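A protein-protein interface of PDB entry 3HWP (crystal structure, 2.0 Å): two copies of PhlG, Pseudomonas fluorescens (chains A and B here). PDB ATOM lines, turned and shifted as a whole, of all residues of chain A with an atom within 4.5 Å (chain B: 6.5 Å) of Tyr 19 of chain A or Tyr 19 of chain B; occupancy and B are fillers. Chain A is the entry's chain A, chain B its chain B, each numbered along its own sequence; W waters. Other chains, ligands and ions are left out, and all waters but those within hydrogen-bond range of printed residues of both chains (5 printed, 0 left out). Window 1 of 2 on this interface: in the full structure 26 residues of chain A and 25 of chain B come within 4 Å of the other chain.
N of Thr 18 of chain A lies within hydrogen-bond range of OG1 of Thr 18 of chain B (3.0 Å).
The backbone NH (N) of Phe 20 of chain B is in hydrogen-bond range of the side-chain hydroxyl (OH) of Tyr 273 of chain A (3.3 Å).
The backbone NH (N) of Phe 20 of chain A is in hydrogen-bond range of the side-chain hydroxyl (OH) of Tyr 273 of chain B (3.3 Å).
The side-chain carboxylate (OE2) of Glu 274 of chain B sits at hydrogen-bond distance from the side-chain hydroxyl (OH) of Tyr 19 of chain A, at 2.6 Å.
The backbone carbonyl oxygen (O) of Thr 18 of chain A sits at hydrogen-bond distance from the side-chain amide nitrogen (NE2) of Gln 59 of chain B, at 3.3 Å.
OH of Tyr 19 of chain B lies within hydrogen-bond range of OE2 of Glu 274 of chain A, 2.5 Å away.
The backbone carbonyl oxygen of Phe 20 of chain B lies within hydrogen-bond range of the side-chain amide nitrogen of Gln 25 of chain B (2.9 Å).
CD1 of Phe 17 of chain A touches OG1 of Thr 18 of chain B (3.3 Å).
Phe 17 of chain A touches Tyr 19 of chain B (CE2 to CB, 3.9 Å).
Phe 17 of chain A touches Gln 59 of chain B.
Thr 18 of chain A touches Pro 16 of chain B (CG2 to O, 3.5 Å).
OG1 of Thr 18 of chain A touches CD1 of Phe 17 of chain B (3.2 Å).
Thr 18 of chain A touches Val 55 of chain B (O to CG2, 3.6 Å).
Tyr 19 of chain A touches Phe 17 of chain B (CB to CZ, 3.8 Å).
CB of Tyr 19 of chain B touches CB of Tyr 19 of chain A (3.4 Å).
Tyr 19 of chain A touches Tyr 273 of chain B (CD1 to OH, 3.4 Å).
Gln 25 of chain B touches Tyr 273 of chain A.
Tyr 19 of chain A touches just these residues of chain B: Phe 17, Tyr 19, Tyr 273 and Glu 274.
Printed residues of chain A within 4 Å of Glu 274 of chain B: Tyr 19.
Of the printed residues of chain A, Phe 20 of chain B touches Tyr 273.
Gly 171 of chain B touches none of the printed residues of chain A.
Cys 281 of chain B touches none of the printed residues of chain A.
The nearest printed residue of chain A that does not touch Tyr 273 of chain B is Thr 18 of chain A (4.3 Å).
Of the 8 printed residues of chain A, 6 touch a printed residue of chain B.
Hydrophobic or aromatic side chains of chain A within 4 Å of the printed part of chain B: Phe 17, Tyr 19 and Tyr 273.
Printed residues of chain B that touch a printed residue of chain A: Pro 16, Phe 17, Thr 18, Tyr 19, Phe 20, Gln 25, Val 55, Gln 59, Tyr 273 and Glu 274.
Phe 17 of chain A touches Tyr 19 of chain B, and with the chains exchanged Tyr 19 of chain A touches Phe 17 of chain B.
Tyr 19 of chain B touches its own counterpart, Tyr 19 of chain A.
Tyr 19 of chain A touches Glu 274 of chain B, and with the chains exchanged Glu 274 of chain A touches Tyr 19 of chain B.
Phe 20 of chain A touches Tyr 273 of chain B, and with the chains exchanged Tyr 273 of chain A touches Phe 20 of chain B.
8 positions are printed for both chains.
Water W1 lies within hydrogen-bond range of the backbone carbonyl oxygen of Thr 18 of chain A and the side-chain hydroxyl of Tyr 273 of chain B.
Water W4 bridges O of Thr 18 of chain B (2.7 Å) and OH of Tyr 273 of chain A (2.7 Å).
Water W2 lies within hydrogen-bond range of OE1 of Glu 274 of chain B (2.8 Å) and OH of Tyr 19 of chain A (3.4 Å).
Water W5 lies within hydrogen-bond range of NE2 of Gln 59 of chain B and O of Phe 17 of chain A.
Water W3 lies within hydrogen-bond range of N of Leu 22 of chain B (2.9 Å) and OE2 of Glu 274 of chain A (3.0 Å).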
ATOM      1  N   PHE A  17      14.097  19.771  -6.849  1.00  0.00           N
ATOM      2  CA  PHE A  17      13.351  19.064  -7.886  1.00  0.00           C
ATOM      3  C   PHE A  17      12.172  18.342  -7.247  1.00  0.00           C
ATOM      4  O   PHE A  17      12.304  17.754  -6.177  1.00  0.00           O
ATOM      5  CB  PHE A  17      14.210  18.078  -8.670  1.00  0.00           C
ATOM      6  CG  PHE A  17      13.806  17.975 -10.108  1.00  0.00           C
ATOM      7  CD1 PHE A  17      14.203  18.946 -11.016  1.00  0.00           C
ATOM      8  CD2 PHE A  17      13.007  16.937 -10.545  1.00  0.00           C
ATOM      9  CE1 PHE A  17      13.823  18.871 -12.341  1.00  0.00           C
ATOM     10  CE2 PHE A  17      12.613  16.855 -11.872  1.00  0.00           C
ATOM     11  CZ  PHE A  17      13.021  17.818 -12.775  1.00  0.00           C
ATOM     12  N   THR A  18      11.024  18.389  -7.916  1.00  0.00           N
ATOM     13  CA  THR A  18       9.759  17.998  -7.300  1.00  0.00           C
ATOM     14  C   THR A  18       9.168  16.714  -7.867  1.00  0.00           C
ATOM     15  O   THR A  18       8.223  16.164  -7.303  1.00  0.00           O
ATOM     16  CB  THR A  18       8.705  19.112  -7.478  1.00  0.00           C
ATOM     17  OG1 THR A  18       8.457  19.309  -8.876  1.00  0.00           O
ATOM     18  CG2 THR A  18       9.202  20.428  -6.874  1.00  0.00           C
ATOM     19  N   TYR A  19       9.711  16.243  -8.984  1.00  0.00           N
ATOM     20  CA  TYR A  19       9.170  15.059  -9.641  1.00  0.00           C
ATOM     21  C   TYR A  19      10.232  13.968  -9.791  1.00  0.00           C
ATOM     22  O   TYR A  19      11.374  14.251 -10.165  1.00  0.00           O
ATOM     23  CB  TYR A  19       8.618  15.445 -11.014  1.00  0.00           C
ATOM     24  CG  TYR A  19       8.137  14.276 -11.864  1.00  0.00           C
ATOM     25  CD1 TYR A  19       6.785  13.954 -11.938  1.00  0.00           C
ATOM     26  CD2 TYR A  19       9.035  13.512 -12.603  1.00  0.00           C
ATOM     27  CE1 TYR A  19       6.335  12.890 -12.727  1.00  0.00           C
ATOM     28  CE2 TYR A  19       8.607  12.452 -13.377  1.00  0.00           C
ATOM     29  CZ  TYR A  19       7.259  12.140 -13.437  1.00  0.00           C
ATOM     30  OH  TYR A  19       6.841  11.082 -14.217  1.00  0.00           O
ATOM     31  N   PHE A  20       9.855  12.729  -9.487  1.00  0.00           N
ATOM     32  CA  PHE A  20      10.716  11.565  -9.733  1.00  0.00           C
ATOM     33  C   PHE A  20       9.826  10.412 -10.188  1.00  0.00           C
ATOM     34  O   PHE A  20       8.884  10.050  -9.486  1.00  0.00           O
ATOM     35  CB  PHE A  20      11.473  11.160  -8.459  1.00  0.00           C
ATOM     36  CG  PHE A  20      12.337  12.257  -7.883  1.00  0.00           C
ATOM     37  CD1 PHE A  20      13.530  12.601  -8.486  1.00  0.00           C
ATOM     38  CD2 PHE A  20      11.944  12.945  -6.742  1.00  0.00           C
ATOM     39  CE1 PHE A  20      14.325  13.616  -7.966  1.00  0.00           C
ATOM     40  CE2 PHE A  20      12.730  13.949  -6.209  1.00  0.00           C
ATOM     41  CZ  PHE A  20      13.921  14.294  -6.824  1.00  0.00           C
ATOM     42  N   SER A  21      10.100   9.831 -11.353  1.00  0.00           N
ATOM     43  CA  SER A  21       9.182   8.828 -11.901  1.00  0.00           C
ATOM     44  C   SER A  21       8.969   7.687 -10.903  1.00  0.00           C
ATOM     45  O   SER A  21       9.802   7.463 -10.013  1.00  0.00           O
ATOM     46  CB  SER A  21       9.681   8.290 -13.248  1.00  0.00           C
ATOM     47  OG  SER A  21      10.868   7.513 -13.093  1.00  0.00           O
ATOM     48  N   TYR A 273      14.941  15.359 -23.322  1.00  0.00           N
ATOM     49  CA  TYR A 273      14.463  16.072 -22.148  1.00  0.00           C
ATOM     50  C   TYR A 273      14.798  15.330 -20.861  1.00  0.00           C
ATOM     51  O   TYR A 273      15.212  15.947 -19.875  1.00  0.00           O
ATOM     52  CB  TYR A 273      12.953  16.320 -22.227  1.00  0.00           C
ATOM     53  CG  TYR A 273      12.377  16.898 -20.949  1.00  0.00           C
ATOM     54  CD1 TYR A 273      12.838  18.104 -20.440  1.00  0.00           C
ATOM     55  CD2 TYR A 273      11.369  16.240 -20.259  1.00  0.00           C
ATOM     56  CE1 TYR A 273      12.317  18.639 -19.270  1.00  0.00           C
ATOM     57  CE2 TYR A 273      10.836  16.768 -19.093  1.00  0.00           C
ATOM     58  CZ  TYR A 273      11.319  17.960 -18.600  1.00  0.00           C
ATOM     59  OH  TYR A 273      10.786  18.482 -17.441  1.00  0.00           O
ATOM     60  N   GLU A 274      14.617  14.012 -20.859  1.00  0.00           N
ATOM     61  CA  GLU A 274      14.894  13.226 -19.657  1.00  0.00           C
ATOM     62  C   GLU A 274      16.390  13.255 -19.300  1.00  0.00           C
ATOM     63  O   GLU A 274      16.751  13.275 -18.116  1.00  0.00           O
ATOM     64  CB  GLU A 274      14.390  11.783 -19.794  1.00  0.00           C
ATOM     65  CG  GLU A 274      12.866  11.656 -20.010  1.00  0.00           C
ATOM     66  CD  GLU A 274      12.027  12.201 -18.853  1.00  0.00           C
ATOM     67  OE1 GLU A 274      12.562  12.363 -17.733  1.00  0.00           O
ATOM     68  OE2 GLU A 274      10.814  12.450 -19.059  1.00  0.00           O
ATOM     69  N   VAL A 277      17.094  16.620 -17.650  1.00  0.00           N
ATOM     70  CA  VAL A 277      16.704  16.587 -16.244  1.00  0.00           C
ATOM     71  C   VAL A 277      17.734  15.800 -15.406  1.00  0.00           C
ATOM     72  O   VAL A 277      18.173  16.255 -14.353  1.00  0.00           O
ATOM     73  CB  VAL A 277      15.304  15.978 -16.076  1.00  0.00           C
ATOM     74  CG1 VAL A 277      15.026  15.659 -14.617  1.00  0.00           C
ATOM     75  CG2 VAL A 277      14.223  16.933 -16.643  1.00  0.00           C
ATOM     76  N   PRO B  16       7.955  25.867  -6.721  1.00  0.00           N
ATOM     77  CA  PRO B  16       7.535  25.683  -8.113  1.00  0.00           C
ATOM     78  C   PRO B  16       7.703  24.236  -8.576  1.00  0.00           C
ATOM     79  O   PRO B  16       8.755  23.625  -8.343  1.00  0.00           O
ATOM     80  CB  PRO B  16       8.488  26.612  -8.884  1.00  0.00           C
ATOM     81  CG  PRO B  16       9.699  26.727  -7.977  1.00  0.00           C
ATOM     82  CD  PRO B  16       9.100  26.791  -6.607  1.00  0.00           C
ATOM     83  N   PHE B  17       6.675  23.681  -9.216  1.00  0.00           N
ATOM     84  CA  PHE B  17       6.837  22.361  -9.809  1.00  0.00           C
ATOM     85  C   PHE B  17       7.873  22.437 -10.934  1.00  0.00           C
ATOM     86  O   PHE B  17       7.860  23.372 -11.743  1.00  0.00           O
ATOM     87  CB  PHE B  17       5.505  21.754 -10.285  1.00  0.00           C
ATOM     88  CG  PHE B  17       5.489  20.254 -10.186  1.00  0.00           C
ATOM     89  CD1 PHE B  17       5.228  19.635  -8.971  1.00  0.00           C
ATOM     90  CD2 PHE B  17       5.805  19.466 -11.279  1.00  0.00           C
ATOM     91  CE1 PHE B  17       5.248  18.250  -8.854  1.00  0.00           C
ATOM     92  CE2 PHE B  17       5.827  18.060 -11.162  1.00  0.00           C
ATOM     93  CZ  PHE B  17       5.556  17.465  -9.954  1.00  0.00           C
ATOM     94  N   THR B  18       8.781  21.469 -10.970  1.00  0.00           N
ATOM     95  CA  THR B  18       9.965  21.570 -11.821  1.00  0.00           C
ATOM     96  C   THR B  18       9.944  20.672 -13.055  1.00  0.00           C
ATOM     97  O   THR B  18      10.837  20.755 -13.891  1.00  0.00           O
ATOM     98  CB  THR B  18      11.235  21.223 -11.037  1.00  0.00           C
ATOM     99  OG1 THR B  18      11.105  19.901 -10.499  1.00  0.00           O
ATOM    100  CG2 THR B  18      11.445  22.213  -9.900  1.00  0.00           C
ATOM    101  N   TYR B  19       8.953  19.798 -13.164  1.00  0.00           N
ATOM    102  CA  TYR B  19       8.948  18.836 -14.262  1.00  0.00           C
ATOM    103  C   TYR B  19       7.621  18.820 -15.025  1.00  0.00           C
ATOM    104  O   TYR B  19       6.559  18.741 -14.413  1.00  0.00           O
ATOM    105  CB  TYR B  19       9.267  17.436 -13.718  1.00  0.00           C
ATOM    106  CG  TYR B  19       9.152  16.323 -14.746  1.00  0.00           C
ATOM    107  CD1 TYR B  19      10.292  15.777 -15.330  1.00  0.00           C
ATOM    108  CD2 TYR B  19       7.910  15.809 -15.121  1.00  0.00           C
ATOM    109  CE1 TYR B  19      10.204  14.763 -16.263  1.00  0.00           C
ATOM    110  CE2 TYR B  19       7.812  14.782 -16.072  1.00  0.00           C
ATOM    111  CZ  TYR B  19       8.973  14.265 -16.629  1.00  0.00           C
ATOM    112  OH  TYR B  19       8.919  13.258 -17.560  1.00  0.00           O
ATOM    113  N   PHE B  20       7.691  18.896 -16.353  1.00  0.00           N
ATOM    114  CA  PHE B  20       6.522  18.694 -17.208  1.00  0.00           C
ATOM    115  C   PHE B  20       6.902  17.821 -18.398  1.00  0.00           C
ATOM    116  O   PHE B  20       7.846  18.141 -19.117  1.00  0.00           O
ATOM    117  CB  PHE B  20       5.940  20.039 -17.689  1.00  0.00           C
ATOM    118  CG  PHE B  20       5.587  20.966 -16.566  1.00  0.00           C
ATOM    119  CD1 PHE B  20       4.427  20.771 -15.836  1.00  0.00           C
ATOM    120  CD2 PHE B  20       6.440  21.990 -16.203  1.00  0.00           C
ATOM    121  CE1 PHE B  20       4.115  21.592 -14.772  1.00  0.00           C
ATOM    122  CE2 PHE B  20       6.126  22.831 -15.142  1.00  0.00           C
ATOM    123  CZ  PHE B  20       4.967  22.626 -14.427  1.00  0.00           C
ATOM    124  N   SER B  21       6.158  16.734 -18.618  1.00  0.00           N
ATOM    125  CA  SER B  21       6.501  15.770 -19.668  1.00  0.00           C
ATOM    126  C   SER B  21       6.609  16.466 -21.013  1.00  0.00           C
ATOM    127  O   SER B  21       5.981  17.497 -21.230  1.00  0.00           O
ATOM    128  CB  SER B  21       5.476  14.630 -19.755  1.00  0.00           C
ATOM    129  OG  SER B  21       4.199  15.106 -20.172  1.00  0.00           O
ATOM    130  N   LEU B  22       7.411  15.895 -21.908  1.00  0.00           N
ATOM    131  CA  LEU B  22       7.596  16.454 -23.244  1.00  0.00           C
ATOM    132  C   LEU B  22       6.278  16.801 -23.954  1.00  0.00           C
ATOM    133  O   LEU B  22       6.100  17.935 -24.390  1.00  0.00           O
ATOM    134  CB  LEU B  22       8.444  15.516 -24.110  1.00  0.00           C
ATOM    135  CG  LEU B  22       8.659  15.945 -25.562  1.00  0.00           C
ATOM    136  CD1 LEU B  22       9.504  17.223 -25.624  1.00  0.00           C
ATOM    137  CD2 LEU B  22       9.303  14.821 -26.365  1.00  0.00           C
ATOM    138  N   MET B  24       3.513  17.459 -22.771  1.00  0.00           N
ATOM    139  CA  MET B  24       2.851  18.525 -22.031  1.00  0.00           C
ATOM    140  C   MET B  24       3.505  19.880 -22.278  1.00  0.00           C
ATOM    141  O   MET B  24       2.830  20.912 -22.273  1.00  0.00           O
ATOM    142  CB  MET B  24       2.799  18.199 -20.540  1.00  0.00           C
ATOM    143  CG  MET B  24       1.597  17.324 -20.169  1.00  0.00           C
ATOM    144  SD  MET B  24       1.619  16.696 -18.316  1.00  0.00           S
ATOM    145  CE  MET B  24       1.652  18.409 -17.387  1.00  0.00           C
ATOM    146  N   GLN B  25       4.816  19.876 -22.511  1.00  0.00           N
ATOM    147  CA  GLN B  25       5.527  21.109 -22.836  1.00  0.00           C
ATOM    148  C   GLN B  25       5.077  21.638 -24.183  1.00  0.00           C
ATOM    149  O   GLN B  25       4.882  22.846 -24.360  1.00  0.00           O
ATOM    150  CB  GLN B  25       7.043  20.883 -22.850  1.00  0.00           C
ATOM    151  CG  GLN B  25       7.623  20.683 -21.480  1.00  0.00           C
ATOM    152  CD  GLN B  25       9.142  20.613 -21.488  1.00  0.00           C
ATOM    153  OE1 GLN B  25       9.817  21.405 -22.152  1.00  0.00           O
ATOM    154  NE2 GLN B  25       9.685  19.676 -20.721  1.00  0.00           N
ATOM    155  N   VAL B  55       4.264  17.737  -1.626  1.00  0.00           N
ATOM    156  CA  VAL B  55       5.007  17.109  -2.710  1.00  0.00           C
ATOM    157  C   VAL B  55       6.053  16.092  -2.199  1.00  0.00           C
ATOM    158  O   VAL B  55       6.266  15.038  -2.806  1.00  0.00           O
ATOM    159  CB  VAL B  55       5.614  18.159  -3.660  1.00  0.00           C
ATOM    160  CG1 VAL B  55       6.916  18.723  -3.089  1.00  0.00           C
ATOM    161  CG2 VAL B  55       5.836  17.554  -5.035  1.00  0.00           C
ATOM    162  N   GLN B  59       7.152  11.517  -3.024  1.00  0.00           N
ATOM    163  CA  GLN B  59       8.438  11.358  -3.688  1.00  0.00           C
ATOM    164  C   GLN B  59       9.173  10.080  -3.301  1.00  0.00           C
ATOM    165  O   GLN B  59      10.211   9.756  -3.879  1.00  0.00           O
ATOM    166  CB  GLN B  59       9.344  12.555  -3.389  1.00  0.00           C
ATOM    167  CG  GLN B  59       8.921  13.824  -4.093  1.00  0.00           C
ATOM    168  CD  GLN B  59       9.739  15.012  -3.653  1.00  0.00           C
ATOM    169  OE1 GLN B  59      10.515  14.925  -2.702  1.00  0.00           O
ATOM    170  NE2 GLN B  59       9.562  16.135  -4.333  1.00  0.00           N
ATOM    171  N   GLY B 171       0.327  12.712 -16.925  1.00  0.00           N
ATOM    172  CA  GLY B 171       1.702  12.301 -17.155  1.00  0.00           C
ATOM    173  C   GLY B 171       2.007  12.538 -18.617  1.00  0.00           C
ATOM    174  O   GLY B 171       1.830  13.649 -19.106  1.00  0.00           O
ATOM    175  N   ASP B 172       2.419  11.500 -19.337  1.00  0.00           N
ATOM    176  CA  ASP B 172       2.653  11.664 -20.769  1.00  0.00           C
ATOM    177  C   ASP B 172       1.522  11.065 -21.611  1.00  0.00           C
ATOM    178  O   ASP B 172       1.632  10.964 -22.834  1.00  0.00           O
ATOM    179  CB  ASP B 172       4.006  11.069 -21.170  1.00  0.00           C
ATOM    180  CG  ASP B 172       4.118   9.610 -20.815  1.00  0.00           C
ATOM    181  OD1 ASP B 172       3.060   8.982 -20.630  1.00  0.00           O
ATOM    182  OD2 ASP B 172       5.254   9.096 -20.717  1.00  0.00           O
ATOM    183  N   TYR B 273       0.434   7.663  -9.308  1.00  0.00           N
ATOM    184  CA  TYR B 273       1.375   8.751  -9.043  1.00  0.00           C
ATOM    185  C   TYR B 273       1.142   9.947  -9.970  1.00  0.00           C
ATOM    186  O   TYR B 273       1.162  11.094  -9.517  1.00  0.00           O
ATOM    187  CB  TYR B 273       2.845   8.284  -9.120  1.00  0.00           C
ATOM    188  CG  TYR B 273       3.855   9.424  -9.056  1.00  0.00           C
ATOM    189  CD1 TYR B 273       3.944  10.239  -7.935  1.00  0.00           C
ATOM    190  CD2 TYR B 273       4.719   9.682 -10.118  1.00  0.00           C
ATOM    191  CE1 TYR B 273       4.862  11.284  -7.874  1.00  0.00           C
ATOM    192  CE2 TYR B 273       5.641  10.719 -10.064  1.00  0.00           C
ATOM    193  CZ  TYR B 273       5.706  11.516  -8.938  1.00  0.00           C
ATOM    194  OH  TYR B 273       6.605  12.559  -8.888  1.00  0.00           O
ATOM    195  N   GLU B 274       0.924   9.698 -11.259  1.00  0.00           N
ATOM    196  CA  GLU B 274       0.755  10.809 -12.189  1.00  0.00           C
ATOM    197  C   GLU B 274      -0.539  11.589 -11.898  1.00  0.00           C
ATOM    198  O   GLU B 274      -0.581  12.810 -12.061  1.00  0.00           O
ATOM    199  CB  GLU B 274       0.821  10.338 -13.646  1.00  0.00           C
ATOM    200  CG  GLU B 274       2.114   9.598 -14.023  1.00  0.00           C
ATOM    201  CD  GLU B 274       3.344  10.500 -14.084  1.00  0.00           C
ATOM    202  OE1 GLU B 274       3.196  11.741 -14.058  1.00  0.00           O
ATOM    203  OE2 GLU B 274       4.473   9.962 -14.158  1.00  0.00           O
ATOM    204  N   VAL B 277       0.253  13.850  -8.889  1.00  0.00           N
ATOM    205  CA  VAL B 277       0.955  15.029  -9.373  1.00  0.00           C
ATOM    206  C   VAL B 277       0.019  16.011 -10.082  1.00  0.00           C
ATOM    207  O   VAL B 277       0.072  17.219  -9.847  1.00  0.00           O
ATOM    208  CB  VAL B 277       2.097  14.645 -10.335  1.00  0.00           C
ATOM    209  CG1 VAL B 277       2.645  15.895 -11.017  1.00  0.00           C
ATOM    210  CG2 VAL B 277       3.202  13.908  -9.576  1.00  0.00           C
ATOM    211  N   CYS B 281      -0.899  19.809  -8.745  1.00  0.00           N
ATOM    212  CA  CYS B 281      -0.538  20.949  -9.578  1.00  0.00           C
ATOM    213  C   CYS B 281      -1.752  21.817  -9.943  1.00  0.00           C
ATOM    214  O   CYS B 281      -1.748  23.032  -9.718  1.00  0.00           O
ATOM    215  CB  CYS B 281       0.187  20.483 -10.852  1.00  0.00           C
ATOM    216  SG  CYS B 281       1.922  19.930 -10.602  1.00  0.00           S
HETATM  217  O   HOH W   1       6.489  14.233  -6.840  1.00  0.00           O
HETATM  218  O   HOH W   2       4.720  12.983 -15.984  1.00  0.00           O
HETATM  219  O   HOH W   3       9.064  13.577 -21.197  1.00  0.00           O
HETATM  220  O   HOH W   4      12.074  20.492 -16.243  1.00  0.00           O
HETATM  221  O   HOH W   5      10.753  18.603  -3.658  1.00  0.00           O
